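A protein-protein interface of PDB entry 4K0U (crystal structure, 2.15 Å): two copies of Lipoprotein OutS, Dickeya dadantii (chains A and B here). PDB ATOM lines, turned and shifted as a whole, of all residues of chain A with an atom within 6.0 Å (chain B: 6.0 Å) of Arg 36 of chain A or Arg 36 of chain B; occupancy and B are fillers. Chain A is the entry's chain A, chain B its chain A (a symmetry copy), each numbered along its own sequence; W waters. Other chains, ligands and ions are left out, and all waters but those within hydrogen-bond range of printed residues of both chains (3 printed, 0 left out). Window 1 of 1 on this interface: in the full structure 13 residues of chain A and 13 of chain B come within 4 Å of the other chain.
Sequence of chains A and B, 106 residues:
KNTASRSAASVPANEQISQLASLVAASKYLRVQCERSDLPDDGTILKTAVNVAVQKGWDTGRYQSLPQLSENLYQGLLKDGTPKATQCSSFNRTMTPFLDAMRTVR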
ATOM      1  N   SER A  27     -15.274   0.102   7.461  1.00  0.00           N
ATOM      2  CA  SER A  27     -14.903   0.778   6.200  1.00  0.00           C
ATOM      3  C   SER A  27     -15.968   0.637   5.119  1.00  0.00           C
ATOM      4  O   SER A  27     -16.198   1.552   4.330  1.00  0.00           O
ATOM      5  CB  SER A  27     -13.604   0.222   5.648  1.00  0.00           C
ATOM      6  OG  SER A  27     -12.557   0.272   6.579  1.00  0.00           O
ATOM      7  N   LEU A  30     -18.705   2.813   6.176  1.00  0.00           N
ATOM      8  CA  LEU A  30     -18.360   4.191   5.720  1.00  0.00           C
ATOM      9  C   LEU A  30     -18.691   4.415   4.267  1.00  0.00           C
ATOM     10  O   LEU A  30     -19.297   5.419   3.847  1.00  0.00           O
ATOM     11  CB  LEU A  30     -16.862   4.457   5.964  1.00  0.00           C
ATOM     12  CG  LEU A  30     -16.449   4.797   7.416  1.00  0.00           C
ATOM     13  CD1 LEU A  30     -14.930   4.907   7.578  1.00  0.00           C
ATOM     14  CD2 LEU A  30     -17.108   6.096   7.828  1.00  0.00           C
ATOM     15  N   ARG A  31     -18.288   3.447   3.455  1.00  0.00           N
ATOM     16  CA  ARG A  31     -18.454   3.589   1.997  1.00  0.00           C
ATOM     17  C   ARG A  31     -19.898   3.732   1.625  1.00  0.00           C
ATOM     18  O   ARG A  31     -20.290   4.627   0.812  1.00  0.00           O
ATOM     19  CB  ARG A  31     -17.829   2.394   1.224  1.00  0.00           C
ATOM     20  CG  ARG A  31     -17.640   2.731  -0.260  1.00  0.00           C
ATOM     21  CD  ARG A  31     -17.103   1.555  -1.111  1.00  0.00           C
ATOM     22  NE  ARG A  31     -17.956   0.370  -0.990  1.00  0.00           N
ATOM     23  CZ  ARG A  31     -17.535  -0.863  -0.669  1.00  0.00           C
ATOM     24  NH1 ARG A  31     -16.251  -1.128  -0.494  1.00  0.00           N
ATOM     25  NH2 ARG A  31     -18.430  -1.859  -0.553  1.00  0.00           N
ATOM     26  N   VAL A  32     -20.714   2.883   2.232  1.00  0.00           N
ATOM     27  CA  VAL A  32     -22.073   2.768   1.813  1.00  0.00           C
ATOM     28  C   VAL A  32     -23.018   3.602   2.667  1.00  0.00           C
ATOM     29  O   VAL A  32     -23.816   4.343   2.143  1.00  0.00           O
ATOM     30  CB  VAL A  32     -22.555   1.309   1.915  1.00  0.00           C
ATOM     31  CG1 VAL A  32     -24.023   1.237   1.446  1.00  0.00           C
ATOM     32  CG2 VAL A  32     -21.680   0.349   1.090  1.00  0.00           C
ATOM     33  N   GLN A  33     -22.998   3.415   3.980  1.00  0.00           N
ATOM     34  CA  GLN A  33     -23.951   4.169   4.814  1.00  0.00           C
ATOM     35  C   GLN A  33     -23.569   5.684   4.922  1.00  0.00           C
ATOM     36  O   GLN A  33     -24.425   6.578   4.806  1.00  0.00           O
ATOM     37  CB  GLN A  33     -24.048   3.549   6.184  1.00  0.00           C
ATOM     38  CG  GLN A  33     -24.528   2.137   6.166  1.00  0.00           C
ATOM     39  CD  GLN A  33     -25.731   1.947   5.286  1.00  0.00           C
ATOM     40  OE1 GLN A  33     -26.684   2.688   5.366  1.00  0.00           O
ATOM     41  NE2 GLN A  33     -25.694   0.941   4.443  1.00  0.00           N
ATOM     42  N   CYS A  34     -22.291   5.963   5.078  1.00  0.00           N
ATOM     43  CA  CYS A  34     -21.810   7.360   5.137  1.00  0.00           C
ATOM     44  C   CYS A  34     -21.355   7.952   3.812  1.00  0.00           C
ATOM     45  O   CYS A  34     -20.830   9.068   3.750  1.00  0.00           O
ATOM     46  CB  CYS A  34     -20.681   7.456   6.181  1.00  0.00           C
ATOM     47  SG  CYS A  34     -21.010   6.434   7.638  1.00  0.00           S
ATOM     48  N   GLU A  35     -21.581   7.250   2.713  1.00  0.00           N
ATOM     49  CA  GLU A  35     -21.283   7.791   1.428  1.00  0.00           C
ATOM     50  C   GLU A  35     -19.851   8.236   1.271  1.00  0.00           C
ATOM     51  O   GLU A  35     -19.539   9.207   0.559  1.00  0.00           O
ATOM     52  CB  GLU A  35     -22.236   8.950   1.052  1.00  0.00           C
ATOM     53  CG  GLU A  35     -23.740   8.702   1.236  1.00  0.00           C
ATOM     54  CD  GLU A  35     -24.365   7.620   0.290  1.00  0.00           C
ATOM     55  OE1 GLU A  35     -23.731   7.210  -0.718  1.00  0.00           O
ATOM     56  OE2 GLU A  35     -25.513   7.187   0.561  1.00  0.00           O
ATOM     57  N   ARG A  36     -18.951   7.497   1.856  1.00  0.00           N
ATOM     58  CA  ARG A  36     -17.542   7.711   1.567  1.00  0.00           C
ATOM     59  C   ARG A  36     -17.136   7.124   0.239  1.00  0.00           C
ATOM     60  O   ARG A  36     -16.422   6.116   0.191  1.00  0.00           O
ATOM     61  CB  ARG A  36     -16.690   7.113   2.668  1.00  0.00           C
ATOM     62  CG  ARG A  36     -16.900   7.792   4.026  1.00  0.00           C
ATOM     63  CD  ARG A  36     -16.345   9.222   4.009  1.00  0.00           C
ATOM     64  NE  ARG A  36     -14.962   9.313   3.582  1.00  0.00           N
ATOM     65  CZ  ARG A  36     -13.904   9.166   4.375  1.00  0.00           C
ATOM     66  NH1 ARG A  36     -14.021   8.950   5.682  1.00  0.00           N
ATOM     67  NH2 ARG A  36     -12.700   9.317   3.862  1.00  0.00           N
ATOM     68  N   SER A  37     -17.539   7.846  -0.806  1.00  0.00           N
ATOM     69  CA  SER A  37     -17.334   7.545  -2.184  1.00  0.00           C
ATOM     70  C   SER A  37     -15.898   7.619  -2.583  1.00  0.00           C
ATOM     71  O   SER A  37     -15.547   7.248  -3.709  1.00  0.00           O
ATOM     72  CB  SER A  37     -18.130   8.491  -3.030  1.00  0.00           C
ATOM     73  OG  SER A  37     -17.786   9.835  -2.759  1.00  0.00           O
ATOM     74  N   ASP A  38     -15.051   8.029  -1.651  1.00  0.00           N
ATOM     75  CA  ASP A  38     -13.638   8.047  -1.890  1.00  0.00           C
ATOM     76  C   ASP A  38     -12.950   6.708  -1.537  1.00  0.00           C
ATOM     77  O   ASP A  38     -11.803   6.503  -1.872  1.00  0.00           O
ATOM     78  CB  ASP A  38     -13.010   9.254  -1.115  1.00  0.00           C
ATOM     79  CG  ASP A  38     -13.244   9.207   0.396  1.00  0.00           C
ATOM     80  OD1 ASP A  38     -14.360   8.969   0.864  1.00  0.00           O
ATOM     81  OD2 ASP A  38     -12.263   9.371   1.141  1.00  0.00           O
ATOM     82  N   LEU A  39     -13.635   5.836  -0.815  1.00  0.00           N
ATOM     83  CA  LEU A  39     -13.128   4.552  -0.397  1.00  0.00           C
ATOM     84  C   LEU A  39     -13.297   3.425  -1.494  1.00  0.00           C
ATOM     85  O   LEU A  39     -14.280   3.400  -2.224  1.00  0.00           O
ATOM     86  CB  LEU A  39     -13.889   4.117   0.850  1.00  0.00           C
ATOM     87  CG  LEU A  39     -13.846   5.102   2.015  1.00  0.00           C
ATOM     88  CD1 LEU A  39     -14.447   4.445   3.254  1.00  0.00           C
ATOM     89  CD2 LEU A  39     -12.404   5.463   2.243  1.00  0.00           C
ATOM     90  N   PRO A  40     -12.352   2.484  -1.553  1.00  0.00           N
ATOM     91  CA  PRO A  40     -12.356   1.505  -2.613  1.00  0.00           C
ATOM     92  C   PRO A  40     -13.200   0.261  -2.295  1.00  0.00           C
ATOM     93  O   PRO A  40     -13.878   0.145  -1.233  1.00  0.00           O
ATOM     94  CB  PRO A  40     -10.876   1.131  -2.689  1.00  0.00           C
ATOM     95  CG  PRO A  40     -10.489   1.073  -1.268  1.00  0.00           C
ATOM     96  CD  PRO A  40     -11.223   2.250  -0.644  1.00  0.00           C
ATOM     97  N   CYS A  88     -21.574   6.913  11.747  1.00  0.00           N
ATOM     98  CA  CYS A  88     -20.681   7.660  10.839  1.00  0.00           C
ATOM     99  C   CYS A  88     -19.742   8.651  11.537  1.00  0.00           C
ATOM    100  O   CYS A  88     -18.604   8.830  11.121  1.00  0.00           O
ATOM    101  CB  CYS A  88     -21.507   8.437   9.803  1.00  0.00           C
ATOM    102  SG  CYS A  88     -22.496   7.397   8.656  1.00  0.00           S
ATOM    103  N   SER A  89     -20.222   9.329  12.571  1.00  0.00           N
ATOM    104  CA  SER A  89     -19.343  10.302  13.333  1.00  0.00           C
ATOM    105  C   SER A  89     -18.249   9.457  14.011  1.00  0.00           C
ATOM    106  O   SER A  89     -17.029   9.750  13.997  1.00  0.00           O
ATOM    107  CB  SER A  89     -20.208  11.120  14.359  1.00  0.00           C
ATOM    108  OG  SER A  89     -19.422  12.008  15.135  1.00  0.00           O
ATOM    109  N   ASN A  92     -15.917   7.695  11.069  1.00  0.00           N
ATOM    110  CA  ASN A  92     -15.109   8.729  10.415  1.00  0.00           C
ATOM    111  C   ASN A  92     -13.910   9.228  11.166  1.00  0.00           C
ATOM    112  O   ASN A  92     -12.895   9.587  10.548  1.00  0.00           O
ATOM    113  CB  ASN A  92     -15.970   9.899  10.018  1.00  0.00           C
ATOM    114  CG  ASN A  92     -16.631   9.701   8.655  1.00  0.00           C
ATOM    115  OD1 ASN A  92     -16.013   9.192   7.709  1.00  0.00           O
ATOM    116  ND2 ASN A  92     -17.856  10.152   8.528  1.00  0.00           N
ATOM    117  N   LEU A  99      -7.749   4.012   6.855  1.00  0.00           N
ATOM    118  CA  LEU A  99      -8.073   4.600   5.590  1.00  0.00           C
ATOM    119  C   LEU A  99      -6.849   5.223   4.920  1.00  0.00           C
ATOM    120  O   LEU A  99      -6.718   5.197   3.703  1.00  0.00           O
ATOM    121  CB  LEU A  99      -9.234   5.599   5.724  1.00  0.00           C
ATOM    122  CG  LEU A  99     -10.542   5.212   6.447  1.00  0.00           C
ATOM    123  CD1 LEU A  99     -11.498   6.401   6.462  1.00  0.00           C
ATOM    124  CD2 LEU A  99     -11.240   4.002   5.820  1.00  0.00           C
ATOM    125  N   SER B  27     -16.529  21.620   2.701  1.00  0.00           N
ATOM    126  CA  SER B  27     -15.810  20.976   3.821  1.00  0.00           C
ATOM    127  C   SER B  27     -16.571  21.063   5.139  1.00  0.00           C
ATOM    128  O   SER B  27     -16.540  20.142   5.954  1.00  0.00           O
ATOM    129  CB  SER B  27     -14.448  21.611   4.029  1.00  0.00           C
ATOM    130  OG  SER B  27     -13.672  21.616   2.861  1.00  0.00           O
ATOM    131  N   LEU B  30     -19.356  18.723   4.797  1.00  0.00           N
ATOM    132  CA  LEU B  30     -18.827  17.371   5.140  1.00  0.00           C
ATOM    133  C   LEU B  30     -18.763  17.139   6.628  1.00  0.00           C
ATOM    134  O   LEU B  30     -19.182  16.105   7.180  1.00  0.00           O
ATOM    135  CB  LEU B  30     -17.427  17.191   4.521  1.00  0.00           C
ATOM    136  CG  LEU B  30     -17.378  16.864   3.009  1.00  0.00           C
ATOM    137  CD1 LEU B  30     -15.947  16.842   2.464  1.00  0.00           C
ATOM    138  CD2 LEU B  30     -18.043  15.527   2.768  1.00  0.00           C
ATOM    139  N   ARG B  31     -18.224  18.135   7.317  1.00  0.00           N
ATOM    140  CA  ARG B  31     -18.004  17.994   8.769  1.00  0.00           C
ATOM    141  C   ARG B  31     -19.295  17.771   9.495  1.00  0.00           C
ATOM    142  O   ARG B  31     -19.414  16.860  10.375  1.00  0.00           O
ATOM    143  CB  ARG B  31     -17.273  19.230   9.365  1.00  0.00           C
ATOM    144  CG  ARG B  31     -16.693  18.915  10.750  1.00  0.00           C
ATOM    145  CD  ARG B  31     -16.027  20.128  11.445  1.00  0.00           C
ATOM    146  NE  ARG B  31     -16.951  21.260  11.554  1.00  0.00           N
ATOM    147  CZ  ARG B  31     -16.697  22.512  11.146  1.00  0.00           C
ATOM    148  NH1 ARG B  31     -15.519  22.851  10.652  1.00  0.00           N
ATOM    149  NH2 ARG B  31     -17.649  23.454  11.270  1.00  0.00           N
ATOM    150  N   VAL B  32     -20.287  18.566   9.122  1.00  0.00           N
ATOM    151  CA  VAL B  32     -21.499  18.605   9.874  1.00  0.00           C
ATOM    152  C   VAL B  32     -22.579  17.711   9.283  1.00  0.00           C
ATOM    153  O   VAL B  32     -23.172  16.929   9.987  1.00  0.00           O
ATOM    154  CB  VAL B  32     -22.074  20.032   9.909  1.00  0.00           C
ATOM    155  CG1 VAL B  32     -23.376  20.022  10.738  1.00  0.00           C
ATOM    156  CG2 VAL B  32     -21.076  21.048  10.492  1.00  0.00           C
ATOM    157  N   GLN B  33     -22.905  17.888   8.009  1.00  0.00           N
ATOM    158  CA  GLN B  33     -23.993  17.074   7.439  1.00  0.00           C
ATOM    159  C   GLN B  33     -23.564  15.583   7.227  1.00  0.00           C
ATOM    160  O   GLN B  33     -24.309  14.642   7.550  1.00  0.00           O
ATOM    161  CB  GLN B  33     -24.473  17.677   6.145  1.00  0.00           C
ATOM    162  CG  GLN B  33     -25.014  19.059   6.295  1.00  0.00           C
ATOM    163  CD  GLN B  33     -25.961  19.185   7.455  1.00  0.00           C
ATOM    164  OE1 GLN B  33     -26.859  18.389   7.613  1.00  0.00           O
ATOM    165  NE2 GLN B  33     -25.770  20.197   8.267  1.00  0.00           N
ATOM    166  N   CYS B  34     -22.353  15.378   6.748  1.00  0.00           N
ATOM    167  CA  CYS B  34     -21.823  14.011   6.558  1.00  0.00           C
ATOM    168  C   CYS B  34     -21.011  13.456   7.720  1.00  0.00           C
ATOM    169  O   CYS B  34     -20.425  12.373   7.637  1.00  0.00           O
ATOM    170  CB  CYS B  34     -20.994  13.973   5.260  1.00  0.00           C
ATOM    171  SG  CYS B  34     -21.742  14.963   3.943  1.00  0.00           S
ATOM    172  N   GLU B  35     -20.991  14.152   8.845  1.00  0.00           N
ATOM    173  CA  GLU B  35     -20.345  13.640  10.007  1.00  0.00           C
ATOM    174  C   GLU B  35     -18.897  13.280   9.790  1.00  0.00           C
ATOM    175  O   GLU B  35     -18.358  12.334  10.393  1.00  0.00           O
ATOM    176  CB  GLU B  35     -21.101  12.430  10.605  1.00  0.00           C
ATOM    177  CG  GLU B  35     -22.614  12.588  10.812  1.00  0.00           C
ATOM    178  CD  GLU B  35     -23.039  13.638  11.894  1.00  0.00           C
ATOM    179  OE1 GLU B  35     -22.195  14.093  12.709  1.00  0.00           O
ATOM    180  OE2 GLU B  35     -24.242  14.003  11.928  1.00  0.00           O
ATOM    181  N   ARG B  36     -18.220  14.066   9.001  1.00  0.00           N
ATOM    182  CA  ARG B  36     -16.773  13.936   8.921  1.00  0.00           C
ATOM    183  C   ARG B  36     -16.078  14.556  10.106  1.00  0.00           C
ATOM    184  O   ARG B  36     -15.436  15.605   9.978  1.00  0.00           O
ATOM    185  CB  ARG B  36     -16.267  14.575   7.644  1.00  0.00           C
ATOM    186  CG  ARG B  36     -16.775  13.875   6.378  1.00  0.00           C
ATOM    187  CD  ARG B  36     -16.152  12.479   6.243  1.00  0.00           C
ATOM    188  NE  ARG B  36     -14.703  12.472   6.303  1.00  0.00           N
ATOM    189  CZ  ARG B  36     -13.893  12.675   5.268  1.00  0.00           C
ATOM    190  NH1 ARG B  36     -14.351  12.873   4.036  1.00  0.00           N
ATOM    191  NH2 ARG B  36     -12.591  12.598   5.456  1.00  0.00           N
ATOM    192  N   SER B  37     -16.158  13.820  11.213  1.00  0.00           N
ATOM    193  CA  SER B  37     -15.628  14.142  12.496  1.00  0.00           C
ATOM    194  C   SER B  37     -14.135  14.156  12.516  1.00  0.00           C
ATOM    195  O   SER B  37     -13.531  14.555  13.518  1.00  0.00           O
ATOM    196  CB  SER B  37     -16.125  13.158  13.510  1.00  0.00           C
ATOM    197  OG  SER B  37     -15.783  11.834  13.151  1.00  0.00           O
ATOM    198  N   ASP B  38     -13.531  13.789  11.396  1.00  0.00           N
ATOM    199  CA  ASP B  38     -12.106  13.854  11.267  1.00  0.00           C
ATOM    200  C   ASP B  38     -11.610  15.228  10.760  1.00  0.00           C
ATOM    201  O   ASP B  38     -10.428  15.503  10.794  1.00  0.00           O
ATOM    202  CB  ASP B  38     -11.627  12.680  10.348  1.00  0.00           C
ATOM    203  CG  ASP B  38     -12.240  12.702   8.948  1.00  0.00           C
ATOM    204  OD1 ASP B  38     -13.450  12.871   8.781  1.00  0.00           O
ATOM    205  OD2 ASP B  38     -11.472  12.591   7.975  1.00  0.00           O
ATOM    206  N   LEU B  39     -12.505  16.055  10.243  1.00  0.00           N
ATOM    207  CA  LEU B  39     -12.198  17.362   9.720  1.00  0.00           C
ATOM    208  C   LEU B  39     -12.146  18.486  10.832  1.00  0.00           C
ATOM    209  O   LEU B  39     -12.911  18.458  11.788  1.00  0.00           O
ATOM    210  CB  LEU B  39     -13.275  17.743   8.710  1.00  0.00           C
ATOM    211  CG  LEU B  39     -13.472  16.752   7.567  1.00  0.00           C
ATOM    212  CD1 LEU B  39     -14.407  17.364   6.525  1.00  0.00           C
ATOM    213  CD2 LEU B  39     -12.117  16.475   6.976  1.00  0.00           C
ATOM    214  N   PRO B  40     -11.274  19.481  10.656  1.00  0.00           N
ATOM    215  CA  PRO B  40     -11.064  20.465  11.689  1.00  0.00           C
ATOM    216  C   PRO B  40     -12.033  21.656  11.605  1.00  0.00           C
ATOM    217  O   PRO B  40     -12.965  21.724  10.753  1.00  0.00           O
ATOM    218  CB  PRO B  40      -9.639  20.926  11.388  1.00  0.00           C
ATOM    219  CG  PRO B  40      -9.631  20.995   9.916  1.00  0.00           C
ATOM    220  CD  PRO B  40     -10.430  19.773   9.490  1.00  0.00           C
ATOM    221  N   CYS B  88     -23.305  14.421   0.110  1.00  0.00           N
ATOM    222  CA  CYS B  88     -22.168  13.734   0.754  1.00  0.00           C
ATOM    223  C   CYS B  88     -21.381  12.794  -0.167  1.00  0.00           C
ATOM    224  O   CYS B  88     -20.167  12.685  -0.056  1.00  0.00           O
ATOM    225  CB  CYS B  88     -22.657  12.917   1.961  1.00  0.00           C
ATOM    226  SG  CYS B  88     -23.380  13.907   3.330  1.00  0.00           S
ATOM    227  N   SER B  89     -22.068  12.082  -1.050  1.00  0.00           N
ATOM    228  CA  SER B  89     -21.357  11.156  -2.018  1.00  0.00           C
ATOM    229  C   SER B  89     -20.523  12.058  -2.946  1.00  0.00           C
ATOM    230  O   SER B  89     -19.325  11.838  -3.245  1.00  0.00           O
ATOM    231  CB  SER B  89     -22.406  10.281  -2.796  1.00  0.00           C
ATOM    232  OG  SER B  89     -21.793   9.434  -3.753  1.00  0.00           O
ATOM    233  N   ASN B  92     -17.626  13.976  -0.681  1.00  0.00           N
ATOM    234  CA  ASN B  92     -16.620  12.995  -0.263  1.00  0.00           C
ATOM    235  C   ASN B  92     -15.624  12.561  -1.298  1.00  0.00           C
ATOM    236  O   ASN B  92     -14.466  12.267  -0.962  1.00  0.00           O
ATOM    237  CB  ASN B  92     -17.280  11.779   0.332  1.00  0.00           C
ATOM    238  CG  ASN B  92     -17.584  11.950   1.820  1.00  0.00           C
ATOM    239  OD1 ASN B  92     -16.776  12.500   2.580  1.00  0.00           O
ATOM    240  ND2 ASN B  92     -18.707  11.429   2.251  1.00  0.00           N
ATOM    241  N   LEU B  99      -8.883  18.160   1.341  1.00  0.00           N
ATOM    242  CA  LEU B  99      -8.840  17.564   2.643  1.00  0.00           C
ATOM    243  C   LEU B  99      -7.451  17.019   2.974  1.00  0.00           C
ATOM    244  O   LEU B  99      -7.017  17.061   4.117  1.00  0.00           O
ATOM    245  CB  LEU B  99      -9.937  16.498   2.801  1.00  0.00           C
ATOM    246  CG  LEU B  99     -11.406  16.802   2.438  1.00  0.00           C
ATOM    247  CD1 LEU B  99     -12.263  15.560   2.658  1.00  0.00           C
ATOM    248  CD2 LEU B  99     -11.990  17.974   3.231  1.00  0.00           C
HETATM  249  O   HOH W   1     -19.606  13.938  13.505  1.00  0.00           O
HETATM  250  O   HOH W   2     -21.443   7.510  -2.145  1.00  0.00           O
HETATM  251  O   HOH W   3     -19.244  10.763   5.515  1.00  0.00           O
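NH1 of Arg 36 of chain B sits at hydrogen-bond distance from OD1 of Asn 92 of chain B (2.9 Å).
The backbone NH of Arg 36 of chain B is in hydrogen-bond range of the backbone carbonyl oxygen of Leu 30 of chain B, at 2.9 Å.
The side-chain amide oxygen of Asn 92 of chain A sits at hydrogen-bond distance from the guanidinium group of Arg 36 of chain A (2.9 Å).
The backbone NH (N) of Glu 35 of chain A lies within hydrogen-bond range of the backbone carbonyl oxygen (O) of Leu 30 of chain A (3.1 Å).
The side-chain sulfur (SG) of Cys 34 of chain B forms a disulfide with the side-chain sulfur (SG) of Cys 88 of chain B, 2.0 Å away.
The backbone carbonyl oxygen (O) of Cys 88 of chain B sits at hydrogen-bond distance from the side-chain amide nitrogen (ND2) of Asn 92 of chain B (3.0 Å).
Of the printed residues of chain B, Cys 34 of chain A touches Asn 92 (3.5 Å).
Of the printed residues of chain B, Glu 35 of chain A touches Cys 88, Ser 89 and Asn 92.
Arg 36 of chain A touches just these residues of chain B: Arg 36 (3.6 Å) and Asn 92 (3.6 Å).
Val 32 of chain B touches none of the printed residues of chain A.
Of the printed residues of chain A, Arg 36 of chain B touches Arg 36 (3.6 Å) and Asn 92 (3.6 Å).
The nearest residue of chain B that does not touch Arg 36 of chain A is Asp 38 of chain B (5.0 Å).
Water W2 bridges the side-chain hydroxyl (OG) of Ser 89 of chain B (2.5 Å) and the side-chain carboxylate (OE1) of Glu 35 of chain A (2.7 Å).
Water W1 bridges OG of Ser 89 of chain A (2.5 Å) and OE1 of Glu 35 of chain B (2.7 Å).
Water W3 lies within hydrogen-bond range of the backbone carbonyl oxygen of Cys 34 of chain B (2.9 Å), the backbone carbonyl oxygen of Cys 34 of chain A (2.9 Å), the side-chain amide nitrogen of Asn 92 of chain A (3.4 Å) and the side-chain amide nitrogen of Asn 92 of chain B (3.4 Å).
Cys 34 of chain A touches Asn 92 of chain B, and with the chains exchanged Asn 92 of chain A touches Cys 34 of chain B.
Glu 35 of chain A touches Asn 92 of chain B, and with the chains exchanged Asn 92 of chain A touches Glu 35 of chain B.
Arg 36 of chain B touches its own counterpart, Arg 36 of chain A.
Arg 36 of chain A touches Asn 92 of chain B, and with the chains exchanged Asn 92 of chain A touches Arg 36 of chain B.
16 positions are printed for both chains.
Of the 16 printed residues of chain A, 8 touch a printed residue of chain B.
Printed residues of chain A that touch a printed residue of chain B: Cys 34, Glu 35, Arg 36, Ser 37, Asp 38, Cys 88, Ser 89 and Asn 92.
Among the printed residues, no Asp or Glu carboxylate lies within 4 Å of a Lys or Arg side-chain nitrogen of the other chain.
Among the printed residues, merely in contact across the chains: Asn 92 of chain A with Asp 38 of chain B (3.3 Å), Asp 38 of chain A with Asn 92 of chain B (3.3 Å), Asn 92 of chain A with Cys 34 of chain B (3.5 Å), Cys 34 of chain A with Asn 92 of chain B (3.5 Å), Cys 88 of chain A with Glu 35 of chain B (3.6 Å), Glu 35 of chain A with Cys 88 of chain B (3.6 Å), Asn 92 of chain A with Arg 36 of chain B (3.6 Å), Arg 36 of chain A with Asn 92 of chain B (3.6 Å), Arg 36 of chain A with Arg 36 of chain B (3.6 Å), Ser 37 of chain A with Asn 92 of chain B (3.7 Å), Asn 92 of chain A with Ser 37 of chain B (3.7 Å), Ser 89 of chain A with Glu 35 of chain B (3.7 Å) and Glu 35 of chain A with Ser 89 of chain B (3.7 Å).
ND2 of Asn 92 of chain A is in hydrogen-bond range of O of Glu 35 of chain B, 2.9 Å away.
O of Glu 35 of chain A lies within hydrogen-bond range of ND2 of Asn 92 of chain B (2.9 Å).
OG of Ser 37 of chain A is in hydrogen-bond range of O of Ser 89 of chain B, 2.6 Å away.
O of Ser 89 of chain A lies within hydrogen-bond range of OG of Ser 37 of chain B (2.6 Å).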
